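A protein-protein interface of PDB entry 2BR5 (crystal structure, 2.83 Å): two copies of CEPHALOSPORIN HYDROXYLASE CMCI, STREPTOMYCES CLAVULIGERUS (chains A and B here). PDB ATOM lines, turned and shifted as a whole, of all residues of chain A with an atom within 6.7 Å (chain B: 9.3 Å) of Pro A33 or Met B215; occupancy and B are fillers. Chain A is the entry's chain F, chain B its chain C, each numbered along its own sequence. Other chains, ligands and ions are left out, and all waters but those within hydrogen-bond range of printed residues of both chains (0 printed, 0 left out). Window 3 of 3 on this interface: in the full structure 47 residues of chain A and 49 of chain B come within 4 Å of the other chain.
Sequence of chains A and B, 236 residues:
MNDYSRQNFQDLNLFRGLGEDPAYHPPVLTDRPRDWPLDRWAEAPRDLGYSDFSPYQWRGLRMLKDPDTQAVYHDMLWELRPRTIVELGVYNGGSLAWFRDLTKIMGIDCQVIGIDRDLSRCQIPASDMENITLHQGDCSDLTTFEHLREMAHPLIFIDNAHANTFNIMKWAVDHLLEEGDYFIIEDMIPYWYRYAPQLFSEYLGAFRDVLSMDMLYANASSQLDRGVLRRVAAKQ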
ATOM      1  N   LEU A  29     -17.610   2.878   5.523  1.00  0.00           N
ATOM      2  CA  LEU A  29     -18.818   3.487   4.995  1.00  0.00           C
ATOM      3  C   LEU A  29     -18.706   3.754   3.504  1.00  0.00           C
ATOM      4  O   LEU A  29     -17.904   4.592   3.091  1.00  0.00           O
ATOM      5  CB  LEU A  29     -19.077   4.806   5.718  1.00  0.00           C
ATOM      6  CG  LEU A  29     -19.997   4.806   6.943  1.00  0.00           C
ATOM      7  CD1 LEU A  29     -20.136   3.424   7.589  1.00  0.00           C
ATOM      8  CD2 LEU A  29     -19.488   5.839   7.951  1.00  0.00           C
ATOM      9  N   THR A  30     -19.532   3.077   2.701  1.00  0.00           N
ATOM     10  CA  THR A  30     -19.440   3.163   1.232  1.00  0.00           C
ATOM     11  C   THR A  30     -20.301   4.257   0.627  1.00  0.00           C
ATOM     12  O   THR A  30     -19.935   4.823  -0.389  1.00  0.00           O
ATOM     13  CB  THR A  30     -19.813   1.825   0.561  1.00  0.00           C
ATOM     14  OG1 THR A  30     -21.208   1.552   0.745  1.00  0.00           O
ATOM     15  CG2 THR A  30     -19.098   0.651   1.226  1.00  0.00           C
ATOM     16  N   ASP A  31     -21.449   4.540   1.225  1.00  0.00           N
ATOM     17  CA  ASP A  31     -22.353   5.541   0.666  1.00  0.00           C
ATOM     18  C   ASP A  31     -22.314   6.872   1.421  1.00  0.00           C
ATOM     19  O   ASP A  31     -22.670   7.886   0.853  1.00  0.00           O
ATOM     20  CB  ASP A  31     -23.793   4.998   0.544  1.00  0.00           C
ATOM     21  CG  ASP A  31     -24.426   4.695   1.889  1.00  0.00           C
ATOM     22  OD1 ASP A  31     -25.128   5.577   2.427  1.00  0.00           O
ATOM     23  OD2 ASP A  31     -24.277   3.607   2.489  1.00  0.00           O
ATOM     24  N   ARG A  32     -21.873   6.887   2.678  1.00  0.00           N
ATOM     25  CA  ARG A  32     -21.754   8.136   3.440  1.00  0.00           C
ATOM     26  C   ARG A  32     -20.301   8.547   3.638  1.00  0.00           C
ATOM     27  O   ARG A  32     -19.419   7.689   3.768  1.00  0.00           O
ATOM     28  CB  ARG A  32     -22.354   8.008   4.852  1.00  0.00           C
ATOM     29  CG  ARG A  32     -23.716   7.388   4.930  1.00  0.00           C
ATOM     30  CD  ARG A  32     -23.682   5.903   5.188  1.00  0.00           C
ATOM     31  NE  ARG A  32     -25.024   5.350   5.248  1.00  0.00           N
ATOM     32  CZ  ARG A  32     -25.829   5.497   6.283  1.00  0.00           C
ATOM     33  NH1 ARG A  32     -25.443   6.164   7.364  1.00  0.00           N
ATOM     34  NH2 ARG A  32     -27.029   4.956   6.245  1.00  0.00           N
ATOM     35  N   PRO A  33     -20.057   9.858   3.706  1.00  0.00           N
ATOM     36  CA  PRO A  33     -18.842  10.356   4.346  1.00  0.00           C
ATOM     37  C   PRO A  33     -19.006  10.166   5.853  1.00  0.00           C
ATOM     38  O   PRO A  33     -20.120  10.237   6.378  1.00  0.00           O
ATOM     39  CB  PRO A  33     -18.832  11.844   3.979  1.00  0.00           C
ATOM     40  CG  PRO A  33     -20.267  12.199   3.821  1.00  0.00           C
ATOM     41  CD  PRO A  33     -20.901  10.967   3.211  1.00  0.00           C
ATOM     42  N   ARG A  34     -17.911   9.899   6.541  1.00  0.00           N
ATOM     43  CA  ARG A  34     -17.970   9.742   7.973  1.00  0.00           C
ATOM     44  C   ARG A  34     -18.348  11.056   8.647  1.00  0.00           C
ATOM     45  O   ARG A  34     -19.129  11.071   9.588  1.00  0.00           O
ATOM     46  CB  ARG A  34     -16.629   9.270   8.491  1.00  0.00           C
ATOM     47  CG  ARG A  34     -16.723   8.495   9.760  1.00  0.00           C
ATOM     48  CD  ARG A  34     -15.416   8.388  10.454  1.00  0.00           C
ATOM     49  NE  ARG A  34     -15.618   8.222  11.879  1.00  0.00           N
ATOM     50  CZ  ARG A  34     -14.860   7.487  12.658  1.00  0.00           C
ATOM     51  NH1 ARG A  34     -13.802   6.846  12.181  1.00  0.00           N
ATOM     52  NH2 ARG A  34     -15.164   7.391  13.935  1.00  0.00           N
ATOM     53  N   ASP A  35     -17.804  12.164   8.161  1.00  0.00           N
ATOM     54  CA  ASP A  35     -18.092  13.461   8.749  1.00  0.00           C
ATOM     55  C   ASP A  35     -19.221  14.157   8.016  1.00  0.00           C
ATOM     56  O   ASP A  35     -19.012  14.817   7.006  1.00  0.00           O
ATOM     57  CB  ASP A  35     -16.835  14.323   8.796  1.00  0.00           C
ATOM     58  CG  ASP A  35     -15.782  13.748   9.729  1.00  0.00           C
ATOM     59  OD1 ASP A  35     -16.138  13.356  10.868  1.00  0.00           O
ATOM     60  OD2 ASP A  35     -14.581  13.627   9.395  1.00  0.00           O
ATOM     61  N   TRP A  36     -20.427  13.996   8.538  1.00  0.00           N
ATOM     62  CA  TRP A  36     -21.597  14.649   7.979  1.00  0.00           C
ATOM     63  C   TRP A  36     -21.723  16.076   8.484  1.00  0.00           C
ATOM     64  O   TRP A  36     -21.803  16.308   9.675  1.00  0.00           O
ATOM     65  CB  TRP A  36     -22.865  13.866   8.326  1.00  0.00           C
ATOM     66  CG  TRP A  36     -24.025  14.233   7.445  1.00  0.00           C
ATOM     67  CD1 TRP A  36     -24.874  15.283   7.608  1.00  0.00           C
ATOM     68  CD2 TRP A  36     -24.446  13.556   6.255  1.00  0.00           C
ATOM     69  NE1 TRP A  36     -25.801  15.293   6.596  1.00  0.00           N
ATOM     70  CE2 TRP A  36     -25.559  14.242   5.754  1.00  0.00           C
ATOM     71  CE3 TRP A  36     -23.990  12.434   5.562  1.00  0.00           C
ATOM     72  CZ2 TRP A  36     -26.226  13.846   4.593  1.00  0.00           C
ATOM     73  CZ3 TRP A  36     -24.658  12.040   4.414  1.00  0.00           C
ATOM     74  CH2 TRP A  36     -25.767  12.740   3.946  1.00  0.00           C
ATOM     75  N   PRO A  37     -21.777  17.033   7.578  1.00  0.00           N
ATOM     76  CA  PRO A  37     -21.864  18.444   7.969  1.00  0.00           C
ATOM     77  C   PRO A  37     -23.191  18.842   8.661  1.00  0.00           C
ATOM     78  O   PRO A  37     -24.266  18.432   8.242  1.00  0.00           O
ATOM     79  CB  PRO A  37     -21.688  19.164   6.641  1.00  0.00           C
ATOM     80  CG  PRO A  37     -22.208  18.190   5.615  1.00  0.00           C
ATOM     81  CD  PRO A  37     -21.775  16.862   6.113  1.00  0.00           C
ATOM     82  N   ALA A  44     -29.190  13.641   6.692  1.00  0.00           N
ATOM     83  CA  ALA A  44     -28.341  12.490   6.923  1.00  0.00           C
ATOM     84  C   ALA A  44     -29.187  11.235   6.946  1.00  0.00           C
ATOM     85  O   ALA A  44     -30.307  11.265   7.448  1.00  0.00           O
ATOM     86  CB  ALA A  44     -27.576  12.643   8.228  1.00  0.00           C
ATOM     87  N   PRO A  45     -28.669  10.138   6.389  1.00  0.00           N
ATOM     88  CA  PRO A  45     -29.378   8.858   6.426  1.00  0.00           C
ATOM     89  C   PRO A  45     -29.400   8.274   7.836  1.00  0.00           C
ATOM     90  O   PRO A  45     -28.408   8.381   8.564  1.00  0.00           O
ATOM     91  CB  PRO A  45     -28.553   7.987   5.475  1.00  0.00           C
ATOM     92  CG  PRO A  45     -27.198   8.524   5.596  1.00  0.00           C
ATOM     93  CD  PRO A  45     -27.388  10.013   5.666  1.00  0.00           C
ATOM     94  N   ARG A  46     -30.526   7.655   8.188  1.00  0.00           N
ATOM     95  CA  ARG A  46     -30.788   7.163   9.535  1.00  0.00           C
ATOM     96  C   ARG A  46     -30.413   5.703   9.768  1.00  0.00           C
ATOM     97  O   ARG A  46     -30.337   5.275  10.924  1.00  0.00           O
ATOM     98  CB  ARG A  46     -32.263   7.360   9.875  1.00  0.00           C
ATOM     99  CG  ARG A  46     -32.689   8.807   9.866  1.00  0.00           C
ATOM    100  CD  ARG A  46     -32.937   9.401  11.237  1.00  0.00           C
ATOM    101  NE  ARG A  46     -34.355   9.346  11.605  1.00  0.00           N
ATOM    102  CZ  ARG A  46     -34.912   8.484  12.478  1.00  0.00           C
ATOM    103  NH1 ARG A  46     -34.189   7.560  13.131  1.00  0.00           N
ATOM    104  NH2 ARG A  46     -36.224   8.551  12.706  1.00  0.00           N
ATOM    105  N   ASP A  47     -30.180   4.929   8.712  1.00  0.00           N
ATOM    106  CA  ASP A  47     -29.768   3.529   8.897  1.00  0.00           C
ATOM    107  C   ASP A  47     -28.269   3.419   9.189  1.00  0.00           C
ATOM    108  O   ASP A  47     -27.525   4.388   9.093  1.00  0.00           O
ATOM    109  CB  ASP A  47     -30.188   2.635   7.716  1.00  0.00           C
ATOM    110  CG  ASP A  47     -29.375   2.894   6.452  1.00  0.00           C
ATOM    111  OD1 ASP A  47     -28.596   1.997   6.053  1.00  0.00           O
ATOM    112  OD2 ASP A  47     -29.455   3.958   5.795  1.00  0.00           O
ATOM    113  N   LEU A  48     -27.838   2.212   9.527  1.00  0.00           N
ATOM    114  CA  LEU A  48     -26.588   2.008  10.252  1.00  0.00           C
ATOM    115  C   LEU A  48     -25.333   2.372   9.477  1.00  0.00           C
ATOM    116  O   LEU A  48     -24.309   2.666  10.096  1.00  0.00           O
ATOM    117  CB  LEU A  48     -26.503   0.550  10.717  1.00  0.00           C
ATOM    118  CG  LEU A  48     -25.329   0.103  11.595  1.00  0.00           C
ATOM    119  CD1 LEU A  48     -25.194   0.981  12.860  1.00  0.00           C
ATOM    120  CD2 LEU A  48     -25.478  -1.388  11.951  1.00  0.00           C
ATOM    121  N   GLY A  49     -25.411   2.335   8.145  1.00  0.00           N
ATOM    122  CA  GLY A  49     -24.265   2.586   7.281  1.00  0.00           C
ATOM    123  C   GLY A  49     -23.460   1.355   6.877  1.00  0.00           C
ATOM    124  O   GLY A  49     -22.562   1.464   6.054  1.00  0.00           O
ATOM    125  N   TYR A  50     -23.763   0.194   7.451  1.00  0.00           N
ATOM    126  CA  TYR A  50     -23.053  -1.049   7.123  1.00  0.00           C
ATOM    127  C   TYR A  50     -23.807  -2.302   7.594  1.00  0.00           C
ATOM    128  O   TYR A  50     -24.829  -2.211   8.285  1.00  0.00           O
ATOM    129  CB  TYR A  50     -21.634  -1.038   7.716  1.00  0.00           C
ATOM    130  CG  TYR A  50     -21.571  -0.768   9.207  1.00  0.00           C
ATOM    131  CD1 TYR A  50     -21.505  -1.807  10.131  1.00  0.00           C
ATOM    132  CD2 TYR A  50     -21.564   0.536   9.692  1.00  0.00           C
ATOM    133  CE1 TYR A  50     -21.446  -1.550  11.494  1.00  0.00           C
ATOM    134  CE2 TYR A  50     -21.510   0.803  11.041  1.00  0.00           C
ATOM    135  CZ  TYR A  50     -21.447  -0.235  11.939  1.00  0.00           C
ATOM    136  OH  TYR A  50     -21.380   0.070  13.285  1.00  0.00           O
ATOM    137  N   VAL B  72     -21.149   0.709  21.293  1.00  0.00           N
ATOM    138  CA  VAL B  72     -20.624   1.858  20.571  1.00  0.00           C
ATOM    139  C   VAL B  72     -19.429   2.462  21.328  1.00  0.00           C
ATOM    140  O   VAL B  72     -18.367   2.637  20.746  1.00  0.00           O
ATOM    141  CB  VAL B  72     -21.724   2.919  20.285  1.00  0.00           C
ATOM    142  CG1 VAL B  72     -21.135   4.165  19.648  1.00  0.00           C
ATOM    143  CG2 VAL B  72     -22.820   2.337  19.378  1.00  0.00           C
ATOM    144  N   TYR B 182     -14.652  14.457  20.945  1.00  0.00           N
ATOM    145  CA  TYR B 182     -16.086  14.260  20.760  1.00  0.00           C
ATOM    146  C   TYR B 182     -16.897  15.119  21.709  1.00  0.00           C
ATOM    147  O   TYR B 182     -16.570  15.209  22.878  1.00  0.00           O
ATOM    148  CB  TYR B 182     -16.449  12.790  21.027  1.00  0.00           C
ATOM    149  CG  TYR B 182     -16.151  11.895  19.869  1.00  0.00           C
ATOM    150  CD1 TYR B 182     -14.838  11.544  19.565  1.00  0.00           C
ATOM    151  CD2 TYR B 182     -17.170  11.407  19.066  1.00  0.00           C
ATOM    152  CE1 TYR B 182     -14.541  10.732  18.484  1.00  0.00           C
ATOM    153  CE2 TYR B 182     -16.891  10.593  17.990  1.00  0.00           C
ATOM    154  CZ  TYR B 182     -15.566  10.266  17.692  1.00  0.00           C
ATOM    155  OH  TYR B 182     -15.281   9.451  16.637  1.00  0.00           O
ATOM    156  N   SER B 212     -18.771  18.151  13.280  1.00  0.00           N
ATOM    157  CA  SER B 212     -19.463  17.301  12.311  1.00  0.00           C
ATOM    158  C   SER B 212     -20.189  16.191  13.065  1.00  0.00           C
ATOM    159  O   SER B 212     -19.906  15.957  14.227  1.00  0.00           O
ATOM    160  CB  SER B 212     -18.468  16.672  11.337  1.00  0.00           C
ATOM    161  OG  SER B 212     -17.632  15.727  12.009  1.00  0.00           O
ATOM    162  N   MET B 213     -21.125  15.518  12.402  1.00  0.00           N
ATOM    163  CA  MET B 213     -21.792  14.372  12.969  1.00  0.00           C
ATOM    164  C   MET B 213     -21.027  13.148  12.484  1.00  0.00           C
ATOM    165  O   MET B 213     -20.819  12.952  11.296  1.00  0.00           O
ATOM    166  CB  MET B 213     -23.255  14.322  12.536  1.00  0.00           C
ATOM    167  CG  MET B 213     -23.985  13.067  12.997  1.00  0.00           C
ATOM    168  SD  MET B 213     -25.782  13.218  13.034  1.00  0.00           S
ATOM    169  CE  MET B 213     -26.133  13.140  11.354  1.00  0.00           C
ATOM    170  N   ASP B 214     -20.583  12.331  13.420  1.00  0.00           N
ATOM    171  CA  ASP B 214     -19.805  11.160  13.088  1.00  0.00           C
ATOM    172  C   ASP B 214     -20.705   9.983  12.742  1.00  0.00           C
ATOM    173  O   ASP B 214     -21.289   9.367  13.637  1.00  0.00           O
ATOM    174  CB  ASP B 214     -18.927  10.798  14.264  1.00  0.00           C
ATOM    175  CG  ASP B 214     -18.020   9.663  13.959  1.00  0.00           C
ATOM    176  OD1 ASP B 214     -18.224   9.001  12.909  1.00  0.00           O
ATOM    177  OD2 ASP B 214     -17.084   9.357  14.717  1.00  0.00           O
ATOM    178  N   MET B 215     -20.777   9.647  11.453  1.00  0.00           N
ATOM    179  CA  MET B 215     -21.723   8.640  10.968  1.00  0.00           C
ATOM    180  C   MET B 215     -21.353   7.206  11.358  1.00  0.00           C
ATOM    181  O   MET B 215     -22.202   6.336  11.293  1.00  0.00           O
ATOM    182  CB  MET B 215     -21.905   8.730   9.450  1.00  0.00           C
ATOM    183  CG  MET B 215     -22.523  10.035   8.931  1.00  0.00           C
ATOM    184  SD  MET B 215     -24.004  10.642   9.801  1.00  0.00           S
ATOM    185  CE  MET B 215     -25.216   9.894   8.905  1.00  0.00           C
ATOM    186  N   LEU B 216     -20.112   6.943  11.761  1.00  0.00           N
ATOM    187  CA  LEU B 216     -19.743   5.589  12.185  1.00  0.00           C
ATOM    188  C   LEU B 216     -20.530   5.205  13.404  1.00  0.00           C
ATOM    189  O   LEU B 216     -20.846   4.032  13.591  1.00  0.00           O
ATOM    190  CB  LEU B 216     -18.253   5.494  12.543  1.00  0.00           C
ATOM    191  CG  LEU B 216     -17.573   4.118  12.549  1.00  0.00           C
ATOM    192  CD1 LEU B 216     -17.716   3.399  11.186  1.00  0.00           C
ATOM    193  CD2 LEU B 216     -16.111   4.301  12.873  1.00  0.00           C
ATOM    194  N   TYR B 217     -20.821   6.197  14.247  1.00  0.00           N
ATOM    195  CA  TYR B 217     -21.522   5.962  15.501  1.00  0.00           C
ATOM    196  C   TYR B 217     -22.930   6.585  15.568  1.00  0.00           C
ATOM    197  O   TYR B 217     -23.801   6.065  16.265  1.00  0.00           O
ATOM    198  CB  TYR B 217     -20.667   6.449  16.669  1.00  0.00           C
ATOM    199  CG  TYR B 217     -19.271   5.881  16.664  1.00  0.00           C
ATOM    200  CD1 TYR B 217     -18.147   6.715  16.742  1.00  0.00           C
ATOM    201  CD2 TYR B 217     -19.060   4.510  16.565  1.00  0.00           C
ATOM    202  CE1 TYR B 217     -16.859   6.178  16.735  1.00  0.00           C
ATOM    203  CE2 TYR B 217     -17.776   3.976  16.553  1.00  0.00           C
ATOM    204  CZ  TYR B 217     -16.696   4.809  16.638  1.00  0.00           C
ATOM    205  OH  TYR B 217     -15.453   4.261  16.588  1.00  0.00           O
ATOM    206  N   ALA B 218     -23.187   7.663  14.838  1.00  0.00           N
ATOM    207  CA  ALA B 218     -24.411   8.428  15.106  1.00  0.00           C
ATOM    208  C   ALA B 218     -25.702   7.641  14.845  1.00  0.00           C
ATOM    209  O   ALA B 218     -26.735   7.986  15.382  1.00  0.00           O
ATOM    210  CB  ALA B 218     -24.411   9.743  14.351  1.00  0.00           C
ATOM    211  N   ASN B 219     -25.641   6.575  14.047  1.00  0.00           N
ATOM    212  CA  ASN B 219     -26.820   5.725  13.804  1.00  0.00           C
ATOM    213  C   ASN B 219     -26.785   4.335  14.477  1.00  0.00           C
ATOM    214  O   ASN B 219     -27.565   3.474  14.137  1.00  0.00           O
ATOM    215  CB  ASN B 219     -27.026   5.594  12.290  1.00  0.00           C
ATOM    216  CG  ASN B 219     -27.514   6.890  11.666  1.00  0.00           C
ATOM    217  OD1 ASN B 219     -28.219   7.675  12.308  1.00  0.00           O
ATOM    218  ND2 ASN B 219     -27.134   7.131  10.424  1.00  0.00           N
ATOM    219  N   ALA B 220     -25.911   4.153  15.465  1.00  0.00           N
ATOM    220  CA  ALA B 220     -25.526   2.829  15.969  1.00  0.00           C
ATOM    221  C   ALA B 220     -26.201   2.476  17.285  1.00  0.00           C
ATOM    222  O   ALA B 220     -26.011   1.386  17.811  1.00  0.00           O
ATOM    223  CB  ALA B 220     -24.034   2.769  16.143  1.00  0.00           C
ATOM    224  N   SER B 221     -26.971   3.399  17.837  1.00  0.00           N
ATOM    225  CA  SER B 221     -27.647   3.127  19.087  1.00  0.00           C
ATOM    226  C   SER B 221     -28.790   4.073  19.268  1.00  0.00           C
ATOM    227  O   SER B 221     -28.732   5.224  18.888  1.00  0.00           O
ATOM    228  CB  SER B 221     -26.679   3.262  20.255  1.00  0.00           C
ATOM    229  OG  SER B 221     -26.970   4.395  21.051  1.00  0.00           O
ATOM    230  N   ASP B 225     -28.297   8.201  19.071  1.00  0.00           N
ATOM    231  CA  ASP B 225     -28.881   8.490  17.752  1.00  0.00           C
ATOM    232  C   ASP B 225     -28.885   9.968  17.358  1.00  0.00           C
ATOM    233  O   ASP B 225     -29.611  10.777  17.934  1.00  0.00           O
ATOM    234  CB  ASP B 225     -30.290   7.880  17.697  1.00  0.00           C
ATOM    235  CG  ASP B 225     -31.164   8.470  16.636  1.00  0.00           C
ATOM    236  OD1 ASP B 225     -30.686   8.804  15.520  1.00  0.00           O
ATOM    237  OD2 ASP B 225     -32.388   8.610  16.866  1.00  0.00           O
ATOM    238  N   ARG B 226     -28.054  10.273  16.362  1.00  0.00           N
ATOM    239  CA  ARG B 226     -27.890  11.592  15.764  1.00  0.00           C
ATOM    240  C   ARG B 226     -27.288  12.631  16.717  1.00  0.00           C
ATOM    241  O   ARG B 226     -27.413  13.829  16.487  1.00  0.00           O
ATOM    242  CB  ARG B 226     -29.203  12.090  15.143  1.00  0.00           C
ATOM    243  CG  ARG B 226     -29.704  11.216  14.015  1.00  0.00           C
ATOM    244  CD  ARG B 226     -31.064  11.620  13.482  1.00  0.00           C
ATOM    245  NE  ARG B 226     -32.187  10.995  14.201  1.00  0.00           N
ATOM    246  CZ  ARG B 226     -33.395  11.563  14.362  1.00  0.00           C
ATOM    247  NH1 ARG B 226     -33.672  12.767  13.850  1.00  0.00           N
ATOM    248  NH2 ARG B 226     -34.345  10.920  15.033  1.00  0.00           N
ATOM    249  N   GLY B 227     -26.590  12.166  17.746  1.00  0.00           N
ATOM    250  CA  GLY B 227     -26.004  13.040  18.736  1.00  0.00           C
ATOM    251  C   GLY B 227     -24.504  12.927  18.856  1.00  0.00           C
ATOM    252  O   GLY B 227     -23.919  13.651  19.663  1.00  0.00           O
ATOM    253  N   VAL B 228     -23.874  12.052  18.071  1.00  0.00           N
ATOM    254  CA  VAL B 228     -22.423  11.854  18.148  1.00  0.00           C
ATOM    255  C   VAL B 228     -21.727  12.832  17.229  1.00  0.00           C
ATOM    256  O   VAL B 228     -21.833  12.709  16.026  1.00  0.00           O
ATOM    257  CB  VAL B 228     -21.975  10.421  17.754  1.00  0.00           C
ATOM    258  CG1 VAL B 228     -20.478  10.230  18.024  1.00  0.00           C
ATOM    259  CG2 VAL B 228     -22.806   9.346  18.501  1.00  0.00           C
ATOM    260  N   LEU B 229     -20.998  13.777  17.818  1.00  0.00           N
ATOM    261  CA  LEU B 229     -20.388  14.907  17.120  1.00  0.00           C
ATOM    262  C   LEU B 229     -18.909  14.971  17.427  1.00  0.00           C
ATOM    263  O   LEU B 229     -18.507  14.661  18.537  1.00  0.00           O
ATOM    264  CB  LEU B 229     -21.029  16.205  17.635  1.00  0.00           C
ATOM    265  CG  LEU B 229     -22.342  16.778  17.070  1.00  0.00           C
ATOM    266  CD1 LEU B 229     -23.351  15.750  16.664  1.00  0.00           C
ATOM    267  CD2 LEU B 229     -22.945  17.695  18.083  1.00  0.00           C
ATOM    268  N   ARG B 230     -18.083  15.406  16.488  1.00  0.00           N
ATOM    269  CA  ARG B 230     -16.649  15.605  16.799  1.00  0.00           C
ATOM    270  C   ARG B 230     -16.041  16.894  16.241  1.00  0.00           C
ATOM    271  O   ARG B 230     -16.406  17.339  15.168  1.00  0.00           O
ATOM    272  CB  ARG B 230     -15.818  14.375  16.380  1.00  0.00           C
ATOM    273  CG  ARG B 230     -15.437  14.301  14.905  1.00  0.00           C
ATOM    274  CD  ARG B 230     -15.642  12.952  14.267  1.00  0.00           C
ATOM    275  NE  ARG B 230     -14.483  12.065  14.392  1.00  0.00           N
ATOM    276  CZ  ARG B 230     -13.925  11.351  13.398  1.00  0.00           C
ATOM    277  NH1 ARG B 230     -14.373  11.389  12.143  1.00  0.00           N
ATOM    278  NH2 ARG B 230     -12.883  10.583  13.677  1.00  0.00           N
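Pro A33 touches just one residue of chain B: Met B215. Printed residues of chain B within 4 Å of Arg A34: Tyr B182, Met B213, Asp B214, Met B215, Leu B216, Tyr B217 and Arg B230. Pro A45 touches just these residues of chain B: Met B215 and Asn B219. Met B215 touches just these residues of chain A: Pro A33 (3.5 Å), Arg A34 (2.9 Å), Trp A36 (3.7 Å), Ala A44 (3.7 Å) and Pro A45 (3.5 Å). Of the printed residues of chain A, Tyr B217 touches Arg A34 (3.5 Å). Of the printed residues of chain A, Arg B226 touches Arg A46 (3.4 Å). Val B228 touches none of the printed residues of chain A. Of the printed residues of chain A, Arg B230 touches Arg A34 (3.4 Å) and Asp A35 (2.9 Å). The nearest residue of chain B that does not touch Pro A33 is Met B213 (5.7 Å).
Hydrophobic or aromatic side chains of chain B that line the printed part of chain A: Tyr B182, Met B213, Met B215, Leu B216, Tyr B217 and Ala B220. Along chain B the printed residues that touch a printed residue of chain A span positions 182 to 230. Of the 16 printed residues of chain A, 10 touch a printed residue of chain B. Among the printed residues, Asp or Glu carboxylates within 4 Å of a Lys or Arg side-chain nitrogen of the other chain: Arg A34 with Asp B214 (2.9 Å) and Asp A35 with Arg B230 (2.9 Å).
No position is printed for both chains.
Among the printed residues, pairs that only touch across the chains: Arg A32 with Asn B219, Pro A33 with Met B215, Arg A34 with Leu B216, Arg A34 with Tyr B217, Asp A35 with Met B213, Trp A36 with Ser B212, Trp A36 with Met B215, Ala A44 with Met B213, Ala A44 with Met B215, Pro A45 with Met B215, Arg A46 with Arg B226, Leu A48 with Asn B219 and Leu A48 with Ala B220.
NH2 of Arg A32 lies within salt-bridge range of OD2 of Asp A47, at 2.7 Å. The backbone NH (N) of Leu B216 sits at hydrogen-bond distance from the side-chain carboxylate (OD1) of Asp B214 (3.0 Å). The side-chain hydroxyl (OH) of Tyr B182 lies within hydrogen-bond range of the side-chain carboxylate (OD2) of Asp B214 (2.6 Å). The side-chain carboxylate (OD1) of Asp A31 is in salt-bridge range of the guanidinium group (NE) of Arg A32 (2.8 Å). OD1 of Asp B225 is in salt-bridge range of NE of Arg B226 (3.0 Å). The backbone NH (N) of Arg B230 sits at hydrogen-bond distance from the backbone carbonyl oxygen (O) of Ser B212 (3.0 Å).
OD1 of Asn B219 sits close to O of Arg A46 (3.5 Å). The side-chain carboxylate (OD1) of Asp A35 lies within hydrogen-bond range of the side-chain hydroxyl (OG) of Ser B212 (3.0 Å). OD2 of Asp B214 lies within salt-bridge range of NH2 of Arg A34 (2.9 Å). The side-chain amide nitrogen (ND2) of Asn B219 sits at hydrogen-bond distance from the backbone carbonyl oxygen (O) of Asp A47. The backbone carbonyl oxygen of Arg A34 sits at hydrogen-bond distance from the backbone NH of Met B215. The backbone NH of Met B213 is in hydrogen-bond range of the backbone carbonyl oxygen of Trp A36, 2.9 Å away. The backbone carbonyl oxygen of Arg A34 lies close to the backbone carbonyl oxygen of Met B213, at 3.1 Å. The backbone carbonyl oxygen of Pro A45 is in hydrogen-bond range of the side-chain amide nitrogen of Asn B219 (2.6 Å). NE of Arg A34 lies close to NH1 of Arg B230 (3.4 Å). OH of Tyr B182 sits at hydrogen-bond distance from NH2 of Arg A34 (3.4 Å). NH1 of Arg B230 lies within salt-bridge range of OD1 of Asp A35 (2.9 Å).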
